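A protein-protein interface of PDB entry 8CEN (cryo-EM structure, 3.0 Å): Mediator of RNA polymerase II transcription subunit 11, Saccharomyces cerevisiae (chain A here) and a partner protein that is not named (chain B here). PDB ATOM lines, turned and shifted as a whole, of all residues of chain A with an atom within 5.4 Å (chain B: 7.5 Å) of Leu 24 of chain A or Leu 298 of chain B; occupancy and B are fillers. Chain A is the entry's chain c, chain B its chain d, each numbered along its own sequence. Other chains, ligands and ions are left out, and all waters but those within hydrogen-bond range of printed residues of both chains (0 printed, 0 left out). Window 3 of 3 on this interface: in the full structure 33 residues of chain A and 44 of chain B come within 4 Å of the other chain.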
ATOM      1  N   LEU A  20       5.431 -15.698 -16.844  1.00  0.00           N
ATOM      2  CA  LEU A  20       6.078 -14.585 -17.531  1.00  0.00           C
ATOM      3  C   LEU A  20       7.505 -14.358 -17.049  1.00  0.00           C
ATOM      4  O   LEU A  20       8.323 -13.819 -17.801  1.00  0.00           O
ATOM      5  CB  LEU A  20       5.255 -13.310 -17.355  1.00  0.00           C
ATOM      6  CG  LEU A  20       4.277 -12.922 -18.467  1.00  0.00           C
ATOM      7  CD1 LEU A  20       3.227 -13.992 -18.699  1.00  0.00           C
ATOM      8  CD2 LEU A  20       3.610 -11.619 -18.097  1.00  0.00           C
ATOM      9  N   CYS A  21       7.814 -14.747 -15.811  1.00  0.00           N
ATOM     10  CA  CYS A  21       9.190 -14.716 -15.333  1.00  0.00           C
ATOM     11  C   CYS A  21      10.029 -15.797 -16.002  1.00  0.00           C
ATOM     12  O   CYS A  21      11.126 -15.524 -16.504  1.00  0.00           O
ATOM     13  CB  CYS A  21       9.215 -14.890 -13.819  1.00  0.00           C
ATOM     14  SG  CYS A  21      10.834 -15.305 -13.164  1.00  0.00           S
ATOM     15  N   SER A  22       9.524 -17.033 -16.026  1.00  0.00           N
ATOM     16  CA  SER A  22      10.248 -18.130 -16.662  1.00  0.00           C
ATOM     17  C   SER A  22      10.281 -18.010 -18.181  1.00  0.00           C
ATOM     18  O   SER A  22      11.040 -18.741 -18.829  1.00  0.00           O
ATOM     19  CB  SER A  22       9.634 -19.470 -16.250  1.00  0.00           C
ATOM     20  OG  SER A  22       8.317 -19.603 -16.749  1.00  0.00           O
ATOM     21  N   MET A  23       9.470 -17.112 -18.748  1.00  0.00           N
ATOM     22  CA  MET A  23       9.535 -16.797 -20.171  1.00  0.00           C
ATOM     23  C   MET A  23      10.928 -16.326 -20.565  1.00  0.00           C
ATOM     24  O   MET A  23      11.480 -16.751 -21.589  1.00  0.00           O
ATOM     25  CB  MET A  23       8.510 -15.712 -20.487  1.00  0.00           C
ATOM     26  CG  MET A  23       8.379 -15.380 -21.941  1.00  0.00           C
ATOM     27  SD  MET A  23       7.773 -16.871 -22.716  1.00  0.00           S
ATOM     28  CE  MET A  23       6.110 -16.820 -22.077  1.00  0.00           C
ATOM     29  N   LEU A  24      11.512 -15.444 -19.754  1.00  0.00           N
ATOM     30  CA  LEU A  24      12.838 -14.922 -20.050  1.00  0.00           C
ATOM     31  C   LEU A  24      13.908 -15.991 -19.878  1.00  0.00           C
ATOM     32  O   LEU A  24      14.893 -15.998 -20.624  1.00  0.00           O
ATOM     33  CB  LEU A  24      13.127 -13.715 -19.162  1.00  0.00           C
ATOM     34  CG  LEU A  24      12.201 -12.536 -19.471  1.00  0.00           C
ATOM     35  CD1 LEU A  24      12.411 -11.391 -18.492  1.00  0.00           C
ATOM     36  CD2 LEU A  24      12.347 -12.080 -20.914  1.00  0.00           C
ATOM     37  N   GLN A  25      13.727 -16.903 -18.917  1.00  0.00           N
ATOM     38  CA  GLN A  25      14.646 -18.029 -18.774  1.00  0.00           C
ATOM     39  C   GLN A  25      14.597 -18.930 -19.999  1.00  0.00           C
ATOM     40  O   GLN A  25      15.639 -19.390 -20.484  1.00  0.00           O
ATOM     41  CB  GLN A  25      14.310 -18.821 -17.505  1.00  0.00           C
ATOM     42  CG  GLN A  25      15.310 -19.914 -17.113  1.00  0.00           C
ATOM     43  CD  GLN A  25      15.054 -21.250 -17.792  1.00  0.00           C
ATOM     44  OE1 GLN A  25      13.917 -21.586 -18.120  1.00  0.00           O
ATOM     45  NE2 GLN A  25      16.117 -22.015 -18.008  1.00  0.00           N
ATOM     46  N   GLU A  26      13.394 -19.192 -20.515  1.00  0.00           N
ATOM     47  CA  GLU A  26      13.272 -20.025 -21.706  1.00  0.00           C
ATOM     48  C   GLU A  26      13.861 -19.339 -22.933  1.00  0.00           C
ATOM     49  O   GLU A  26      14.499 -19.993 -23.766  1.00  0.00           O
ATOM     50  CB  GLU A  26      11.810 -20.399 -21.942  1.00  0.00           C
ATOM     51  CG  GLU A  26      11.230 -21.294 -20.861  1.00  0.00           C
ATOM     52  CD  GLU A  26      11.878 -22.663 -20.834  1.00  0.00           C
ATOM     53  OE1 GLU A  26      12.290 -23.148 -21.907  1.00  0.00           O
ATOM     54  OE2 GLU A  26      11.975 -23.256 -19.738  1.00  0.00           O
ATOM     55  N   ALA A  27      13.666 -18.023 -23.056  1.00  0.00           N
ATOM     56  CA  ALA A  27      14.274 -17.282 -24.160  1.00  0.00           C
ATOM     57  C   ALA A  27      15.797 -17.288 -24.065  1.00  0.00           C
ATOM     58  O   ALA A  27      16.488 -17.446 -25.081  1.00  0.00           O
ATOM     59  CB  ALA A  27      13.741 -15.850 -24.189  1.00  0.00           C
ATOM     60  N   SER A  28      16.333 -17.127 -22.849  1.00  0.00           N
ATOM     61  CA  SER A  28      17.774 -17.208 -22.636  1.00  0.00           C
ATOM     62  C   SER A  28      18.311 -18.580 -23.008  1.00  0.00           C
ATOM     63  O   SER A  28      19.366 -18.691 -23.643  1.00  0.00           O
ATOM     64  CB  SER A  28      18.108 -16.895 -21.178  1.00  0.00           C
ATOM     65  OG  SER A  28      19.497 -17.033 -20.934  1.00  0.00           O
ATOM     66  N   GLN A  29      17.594 -19.638 -22.625  1.00  0.00           N
ATOM     67  CA  GLN A  29      18.049 -20.983 -22.949  1.00  0.00           C
ATOM     68  C   GLN A  29      17.979 -21.240 -24.449  1.00  0.00           C
ATOM     69  O   GLN A  29      18.866 -21.892 -25.006  1.00  0.00           O
ATOM     70  CB  GLN A  29      17.231 -22.017 -22.179  1.00  0.00           C
ATOM     71  CG  GLN A  29      17.850 -23.404 -22.182  1.00  0.00           C
ATOM     72  CD  GLN A  29      19.152 -23.458 -21.407  1.00  0.00           C
ATOM     73  OE1 GLN A  29      19.271 -22.873 -20.330  1.00  0.00           O
ATOM     74  NE2 GLN A  29      20.137 -24.161 -21.951  1.00  0.00           N
ATOM     75  N   SER B 287      23.059 -11.390 -25.702  1.00  0.00           N
ATOM     76  CA  SER B 287      21.619 -11.487 -25.489  1.00  0.00           C
ATOM     77  C   SER B 287      21.283 -12.564 -24.466  1.00  0.00           C
ATOM     78  O   SER B 287      20.392 -12.378 -23.631  1.00  0.00           O
ATOM     79  CB  SER B 287      20.913 -11.769 -26.813  1.00  0.00           C
ATOM     80  OG  SER B 287      20.937 -10.632 -27.657  1.00  0.00           O
ATOM     81  N   LYS B 288      21.991 -13.697 -24.520  1.00  0.00           N
ATOM     82  CA  LYS B 288      21.784 -14.773 -23.553  1.00  0.00           C
ATOM     83  C   LYS B 288      22.090 -14.304 -22.137  1.00  0.00           C
ATOM     84  O   LYS B 288      21.308 -14.547 -21.210  1.00  0.00           O
ATOM     85  CB  LYS B 288      22.658 -15.974 -23.926  1.00  0.00           C
ATOM     86  CG  LYS B 288      22.329 -17.281 -23.206  1.00  0.00           C
ATOM     87  CD  LYS B 288      23.159 -17.506 -21.941  1.00  0.00           C
ATOM     88  CE  LYS B 288      24.624 -17.751 -22.260  1.00  0.00           C
ATOM     89  NZ  LYS B 288      25.423 -17.989 -21.025  1.00  0.00           N
ATOM     90  N   LEU B 290      22.194 -11.191 -21.006  1.00  0.00           N
ATOM     91  CA  LEU B 290      21.249 -10.150 -20.616  1.00  0.00           C
ATOM     92  C   LEU B 290      19.904 -10.746 -20.211  1.00  0.00           C
ATOM     93  O   LEU B 290      19.319 -10.346 -19.194  1.00  0.00           O
ATOM     94  CB  LEU B 290      21.087  -9.158 -21.767  1.00  0.00           C
ATOM     95  CG  LEU B 290      20.836  -7.687 -21.451  1.00  0.00           C
ATOM     96  CD1 LEU B 290      21.904  -7.157 -20.515  1.00  0.00           C
ATOM     97  CD2 LEU B 290      20.847  -6.904 -22.748  1.00  0.00           C
ATOM     98  N   LEU B 291      19.417 -11.727 -20.980  1.00  0.00           N
ATOM     99  CA  LEU B 291      18.170 -12.408 -20.643  1.00  0.00           C
ATOM    100  C   LEU B 291      18.290 -13.180 -19.333  1.00  0.00           C
ATOM    101  O   LEU B 291      17.352 -13.192 -18.529  1.00  0.00           O
ATOM    102  CB  LEU B 291      17.765 -13.345 -21.780  1.00  0.00           C
ATOM    103  CG  LEU B 291      17.183 -12.752 -23.063  1.00  0.00           C
ATOM    104  CD1 LEU B 291      16.910 -13.843 -24.073  1.00  0.00           C
ATOM    105  CD2 LEU B 291      15.907 -11.996 -22.765  1.00  0.00           C
ATOM    106  N   ARG B 292      19.437 -13.826 -19.102  1.00  0.00           N
ATOM    107  CA  ARG B 292      19.639 -14.585 -17.869  1.00  0.00           C
ATOM    108  C   ARG B 292      19.646 -13.671 -16.648  1.00  0.00           C
ATOM    109  O   ARG B 292      19.010 -13.970 -15.628  1.00  0.00           O
ATOM    110  CB  ARG B 292      20.951 -15.370 -17.956  1.00  0.00           C
ATOM    111  CG  ARG B 292      21.238 -16.256 -16.757  1.00  0.00           C
ATOM    112  CD  ARG B 292      20.421 -17.535 -16.801  1.00  0.00           C
ATOM    113  NE  ARG B 292      20.654 -18.282 -18.032  1.00  0.00           N
ATOM    114  CZ  ARG B 292      19.985 -19.370 -18.387  1.00  0.00           C
ATOM    115  NH1 ARG B 292      19.027 -19.873 -17.626  1.00  0.00           N
ATOM    116  NH2 ARG B 292      20.289 -19.972 -19.533  1.00  0.00           N
ATOM    117  N   ALA B 293      20.360 -12.543 -16.739  1.00  0.00           N
ATOM    118  CA  ALA B 293      20.404 -11.596 -15.628  1.00  0.00           C
ATOM    119  C   ALA B 293      19.037 -10.976 -15.369  1.00  0.00           C
ATOM    120  O   ALA B 293      18.634 -10.806 -14.207  1.00  0.00           O
ATOM    121  CB  ALA B 293      21.442 -10.510 -15.904  1.00  0.00           C
ATOM    122  N   SER B 294      18.308 -10.636 -16.439  1.00  0.00           N
ATOM    123  CA  SER B 294      16.965 -10.092 -16.282  1.00  0.00           C
ATOM    124  C   SER B 294      16.026 -11.109 -15.650  1.00  0.00           C
ATOM    125  O   SER B 294      15.210 -10.751 -14.795  1.00  0.00           O
ATOM    126  CB  SER B 294      16.423  -9.639 -17.634  1.00  0.00           C
ATOM    127  OG  SER B 294      16.283 -10.747 -18.504  1.00  0.00           O
ATOM    128  N   PHE B 295      16.136 -12.380 -16.051  1.00  0.00           N
ATOM    129  CA  PHE B 295      15.317 -13.429 -15.452  1.00  0.00           C
ATOM    130  C   PHE B 295      15.623 -13.600 -13.970  1.00  0.00           C
ATOM    131  O   PHE B 295      14.704 -13.763 -13.165  1.00  0.00           O
ATOM    132  CB  PHE B 295      15.520 -14.752 -16.194  1.00  0.00           C
ATOM    133  CG  PHE B 295      15.162 -15.967 -15.378  1.00  0.00           C
ATOM    134  CD1 PHE B 295      13.841 -16.249 -15.068  1.00  0.00           C
ATOM    135  CD2 PHE B 295      16.150 -16.829 -14.926  1.00  0.00           C
ATOM    136  CE1 PHE B 295      13.512 -17.361 -14.317  1.00  0.00           C
ATOM    137  CE2 PHE B 295      15.827 -17.943 -14.173  1.00  0.00           C
ATOM    138  CZ  PHE B 295      14.506 -18.210 -13.872  1.00  0.00           C
ATOM    139  N   ASN B 296      16.905 -13.560 -13.591  1.00  0.00           N
ATOM    140  CA  ASN B 296      17.260 -13.725 -12.182  1.00  0.00           C
ATOM    141  C   ASN B 296      16.743 -12.565 -11.332  1.00  0.00           C
ATOM    142  O   ASN B 296      16.122 -12.779 -10.277  1.00  0.00           O
ATOM    143  CB  ASN B 296      18.775 -13.867 -12.038  1.00  0.00           C
ATOM    144  CG  ASN B 296      19.304 -15.130 -12.686  1.00  0.00           C
ATOM    145  OD1 ASN B 296      18.569 -16.097 -12.884  1.00  0.00           O
ATOM    146  ND2 ASN B 296      20.589 -15.129 -13.021  1.00  0.00           N
ATOM    147  N   LYS B 297      16.976 -11.327 -11.788  1.00  0.00           N
ATOM    148  CA  LYS B 297      16.504 -10.164 -11.039  1.00  0.00           C
ATOM    149  C   LYS B 297      14.983 -10.125 -10.968  1.00  0.00           C
ATOM    150  O   LYS B 297      14.408  -9.864  -9.902  1.00  0.00           O
ATOM    151  CB  LYS B 297      17.044  -8.877 -11.663  1.00  0.00           C
ATOM    152  CG  LYS B 297      18.557  -8.759 -11.633  1.00  0.00           C
ATOM    153  CD  LYS B 297      19.073  -8.689 -10.204  1.00  0.00           C
ATOM    154  CE  LYS B 297      18.720  -7.364  -9.550  1.00  0.00           C
ATOM    155  NZ  LYS B 297      19.288  -7.258  -8.178  1.00  0.00           N
ATOM    156  N   LEU B 298      14.312 -10.421 -12.084  1.00  0.00           N
ATOM    157  CA  LEU B 298      12.859 -10.397 -12.110  1.00  0.00           C
ATOM    158  C   LEU B 298      12.268 -11.539 -11.295  1.00  0.00           C
ATOM    159  O   LEU B 298      11.194 -11.382 -10.709  1.00  0.00           O
ATOM    160  CB  LEU B 298      12.380 -10.446 -13.560  1.00  0.00           C
ATOM    161  CG  LEU B 298      10.884 -10.360 -13.827  1.00  0.00           C
ATOM    162  CD1 LEU B 298      10.388  -9.019 -13.330  1.00  0.00           C
ATOM    163  CD2 LEU B 298      10.616 -10.514 -15.312  1.00  0.00           C
ATOM    164  N   SER B 299      12.963 -12.679 -11.219  1.00  0.00           N
ATOM    165  CA  SER B 299      12.531 -13.764 -10.348  1.00  0.00           C
ATOM    166  C   SER B 299      12.608 -13.360  -8.885  1.00  0.00           C
ATOM    167  O   SER B 299      11.698 -13.667  -8.109  1.00  0.00           O
ATOM    168  CB  SER B 299      13.380 -15.011 -10.598  1.00  0.00           C
ATOM    169  OG  SER B 299      14.720 -14.802 -10.190  1.00  0.00           O
ATOM    170  N   SER B 300      13.687 -12.675  -8.491  1.00  0.00           N
ATOM    171  CA  SER B 300      13.780 -12.187  -7.114  1.00  0.00           C
ATOM    172  C   SER B 300      12.670 -11.186  -6.801  1.00  0.00           C
ATOM    173  O   SER B 300      12.012 -11.275  -5.751  1.00  0.00           O
ATOM    174  CB  SER B 300      15.154 -11.561  -6.872  1.00  0.00           C
ATOM    175  OG  SER B 300      15.316 -10.377  -7.634  1.00  0.00           O
ATOM    176  N   ILE B 301      12.419 -10.253  -7.728  1.00  0.00           N
ATOM    177  CA  ILE B 301      11.376  -9.248  -7.519  1.00  0.00           C
ATOM    178  C   ILE B 301       9.995  -9.897  -7.462  1.00  0.00           C
ATOM    179  O   ILE B 301       9.148  -9.509  -6.650  1.00  0.00           O
ATOM    180  CB  ILE B 301      11.457  -8.158  -8.606  1.00  0.00           C
ATOM    181  CG1 ILE B 301      12.816  -7.454  -8.560  1.00  0.00           C
ATOM    182  CG2 ILE B 301      10.345  -7.138  -8.447  1.00  0.00           C
ATOM    183  CD1 ILE B 301      13.101  -6.754  -7.251  1.00  0.00           C
ATOM    184  N   LEU B 302       9.754 -10.913  -8.293  1.00  0.00           N
ATOM    185  CA  LEU B 302       8.447 -11.559  -8.288  1.00  0.00           C
ATOM    186  C   LEU B 302       8.250 -12.484  -7.093  1.00  0.00           C
ATOM    187  O   LEU B 302       7.114 -12.646  -6.640  1.00  0.00           O
ATOM    188  CB  LEU B 302       8.220 -12.314  -9.598  1.00  0.00           C
ATOM    189  CG  LEU B 302       7.895 -11.386 -10.771  1.00  0.00           C
ATOM    190  CD1 LEU B 302       7.583 -12.169 -12.023  1.00  0.00           C
ATOM    191  CD2 LEU B 302       6.735 -10.466 -10.427  1.00  0.00           C
ATOM    192  N   GLN B 303       9.318 -13.089  -6.560  1.00  0.00           N
ATOM    193  CA  GLN B 303       9.189 -13.780  -5.278  1.00  0.00           C
ATOM    194  C   GLN B 303       8.827 -12.803  -4.169  1.00  0.00           C
ATOM    195  O   GLN B 303       7.980 -13.107  -3.315  1.00  0.00           O
ATOM    196  CB  GLN B 303      10.474 -14.534  -4.925  1.00  0.00           C
ATOM    197  CG  GLN B 303      10.798 -15.706  -5.835  1.00  0.00           C
ATOM    198  CD  GLN B 303      12.090 -16.402  -5.450  1.00  0.00           C
ATOM    199  OE1 GLN B 303      12.791 -15.972  -4.535  1.00  0.00           O
ATOM    200  NE2 GLN B 303      12.410 -17.483  -6.150  1.00  0.00           N
ATOM    201  N   ASN B 304       9.446 -11.617  -4.174  1.00  0.00           N
ATOM    202  CA  ASN B 304       9.082 -10.596  -3.194  1.00  0.00           C
ATOM    203  C   ASN B 304       7.630 -10.149  -3.361  1.00  0.00           C
ATOM    204  O   ASN B 304       6.907  -9.982  -2.371  1.00  0.00           O
ATOM    205  CB  ASN B 304      10.033  -9.405  -3.301  1.00  0.00           C
ATOM    206  CG  ASN B 304      11.387  -9.691  -2.684  1.00  0.00           C
ATOM    207  OD1 ASN B 304      11.547 -10.653  -1.932  1.00  0.00           O
ATOM    208  ND2 ASN B 304      12.369  -8.854  -2.997  1.00  0.00           N
ATOM    209  N   GLU B 305       7.181  -9.976  -4.607  1.00  0.00           N
ATOM    210  CA  GLU B 305       5.799  -9.572  -4.863  1.00  0.00           C
ATOM    211  C   GLU B 305       4.809 -10.657  -4.449  1.00  0.00           C
ATOM    212  O   GLU B 305       3.732 -10.351  -3.925  1.00  0.00           O
ATOM    213  CB  GLU B 305       5.613  -9.234  -6.341  1.00  0.00           C
ATOM    214  CG  GLU B 305       4.388  -8.380  -6.641  1.00  0.00           C
ATOM    215  CD  GLU B 305       4.441  -7.746  -8.015  1.00  0.00           C
ATOM    216  OE1 GLU B 305       5.446  -7.953  -8.722  1.00  0.00           O
ATOM    217  OE2 GLU B 305       3.474  -7.055  -8.394  1.00  0.00           O
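Printed residues of chain B within 4 Å of Leu 24 of chain A: Ser 294 (3.9 Å), Phe 295 (3.95 Å) and Leu 298 (3.8 Å).
Leu 298 of chain B touches just one residue of chain A: Leu 24.
Printed residues of chain B within 4 Å of Ala 27 of chain A: Leu 291.
Of the printed residues of chain A, Arg 292 of chain B touches Gln 25, Ser 28 and Gln 29.
Of the printed residues of chain B, Cys 21 of chain A touches Phe 295 (3.2 Å), Ser 299 (3.6 Å) and Leu 302 (3.6 Å).
Of the printed residues of chain B, Gln 25 of chain A touches Arg 292 (3.6 Å) and Phe 295 (3.6 Å).
Asn 304 of chain B touches none of the printed residues of chain A.
Among the printed residues, merely in contact across the chains: Cys 21 of chain A with Phe 295 of chain B, Cys 21 of chain A with Ser 299 of chain B, Cys 21 of chain A with Leu 302 of chain B, Leu 24 of chain A with Ser 294 of chain B, Leu 24 of chain A with Phe 295 of chain B, Leu 24 of chain A with Leu 298 of chain B, Gln 25 of chain A with Arg 292 of chain B, Gln 25 of chain A with Phe 295 of chain B, Ala 27 of chain A with Leu 291 of chain B and Ser 28 of chain A with Leu 291 of chain B.
The side-chain hydroxyl (OG) of Ser 28 of chain A lies within hydrogen-bond range of the backbone carbonyl oxygen (O) of Lys 288 of chain B (3.1 Å).
The guanidinium group (NH2) of Arg 292 of chain B sits at hydrogen-bond distance from the side-chain hydroxyl (OG) of Ser 28 of chain A, at 3.4 Å.
NH2 of Arg 292 of chain B sits at hydrogen-bond distance from OE1 of Gln 29 of chain A (3.2 Å).
Of the 10 printed residues of chain A, 6 touch a printed residue of chain B.
Hydrophobic or aromatic side chains of chain A within 4 Å of the printed part of chain B: Leu 24 and Ala 27.
Among the printed residues, no Asp or Glu carboxylate lies within 4 Å of a Lys or Arg side-chain nitrogen of the other chain.
The side-chain amide oxygen of Gln 25 of chain A sits close to the side-chain carboxylate of Glu 26 of chain A, 3.0 Å away.
O of Leu 290 of chain B sits at hydrogen-bond distance from OG of Ser 294 of chain B.
The side-chain hydroxyl (OG) of Ser 294 of chain B is in hydrogen-bond range of the backbone carbonyl oxygen (O) of Leu 291 of chain B (2.7 Å).
The side-chain amide nitrogen (ND2) of Asn 296 of chain B sits close to the backbone carbonyl oxygen (O) of Arg 292 of chain B (3.3 Å).
The backbone carbonyl oxygen (O) of Phe 295 of chain B sits close to the side-chain hydroxyl (OG) of Ser 299 of chain B (3.2 Å).
The side-chain hydroxyl (OG) of Ser 299 of chain B is in hydrogen-bond range of the backbone carbonyl oxygen (O) of Asn 296 of chain B (2.5 Å).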
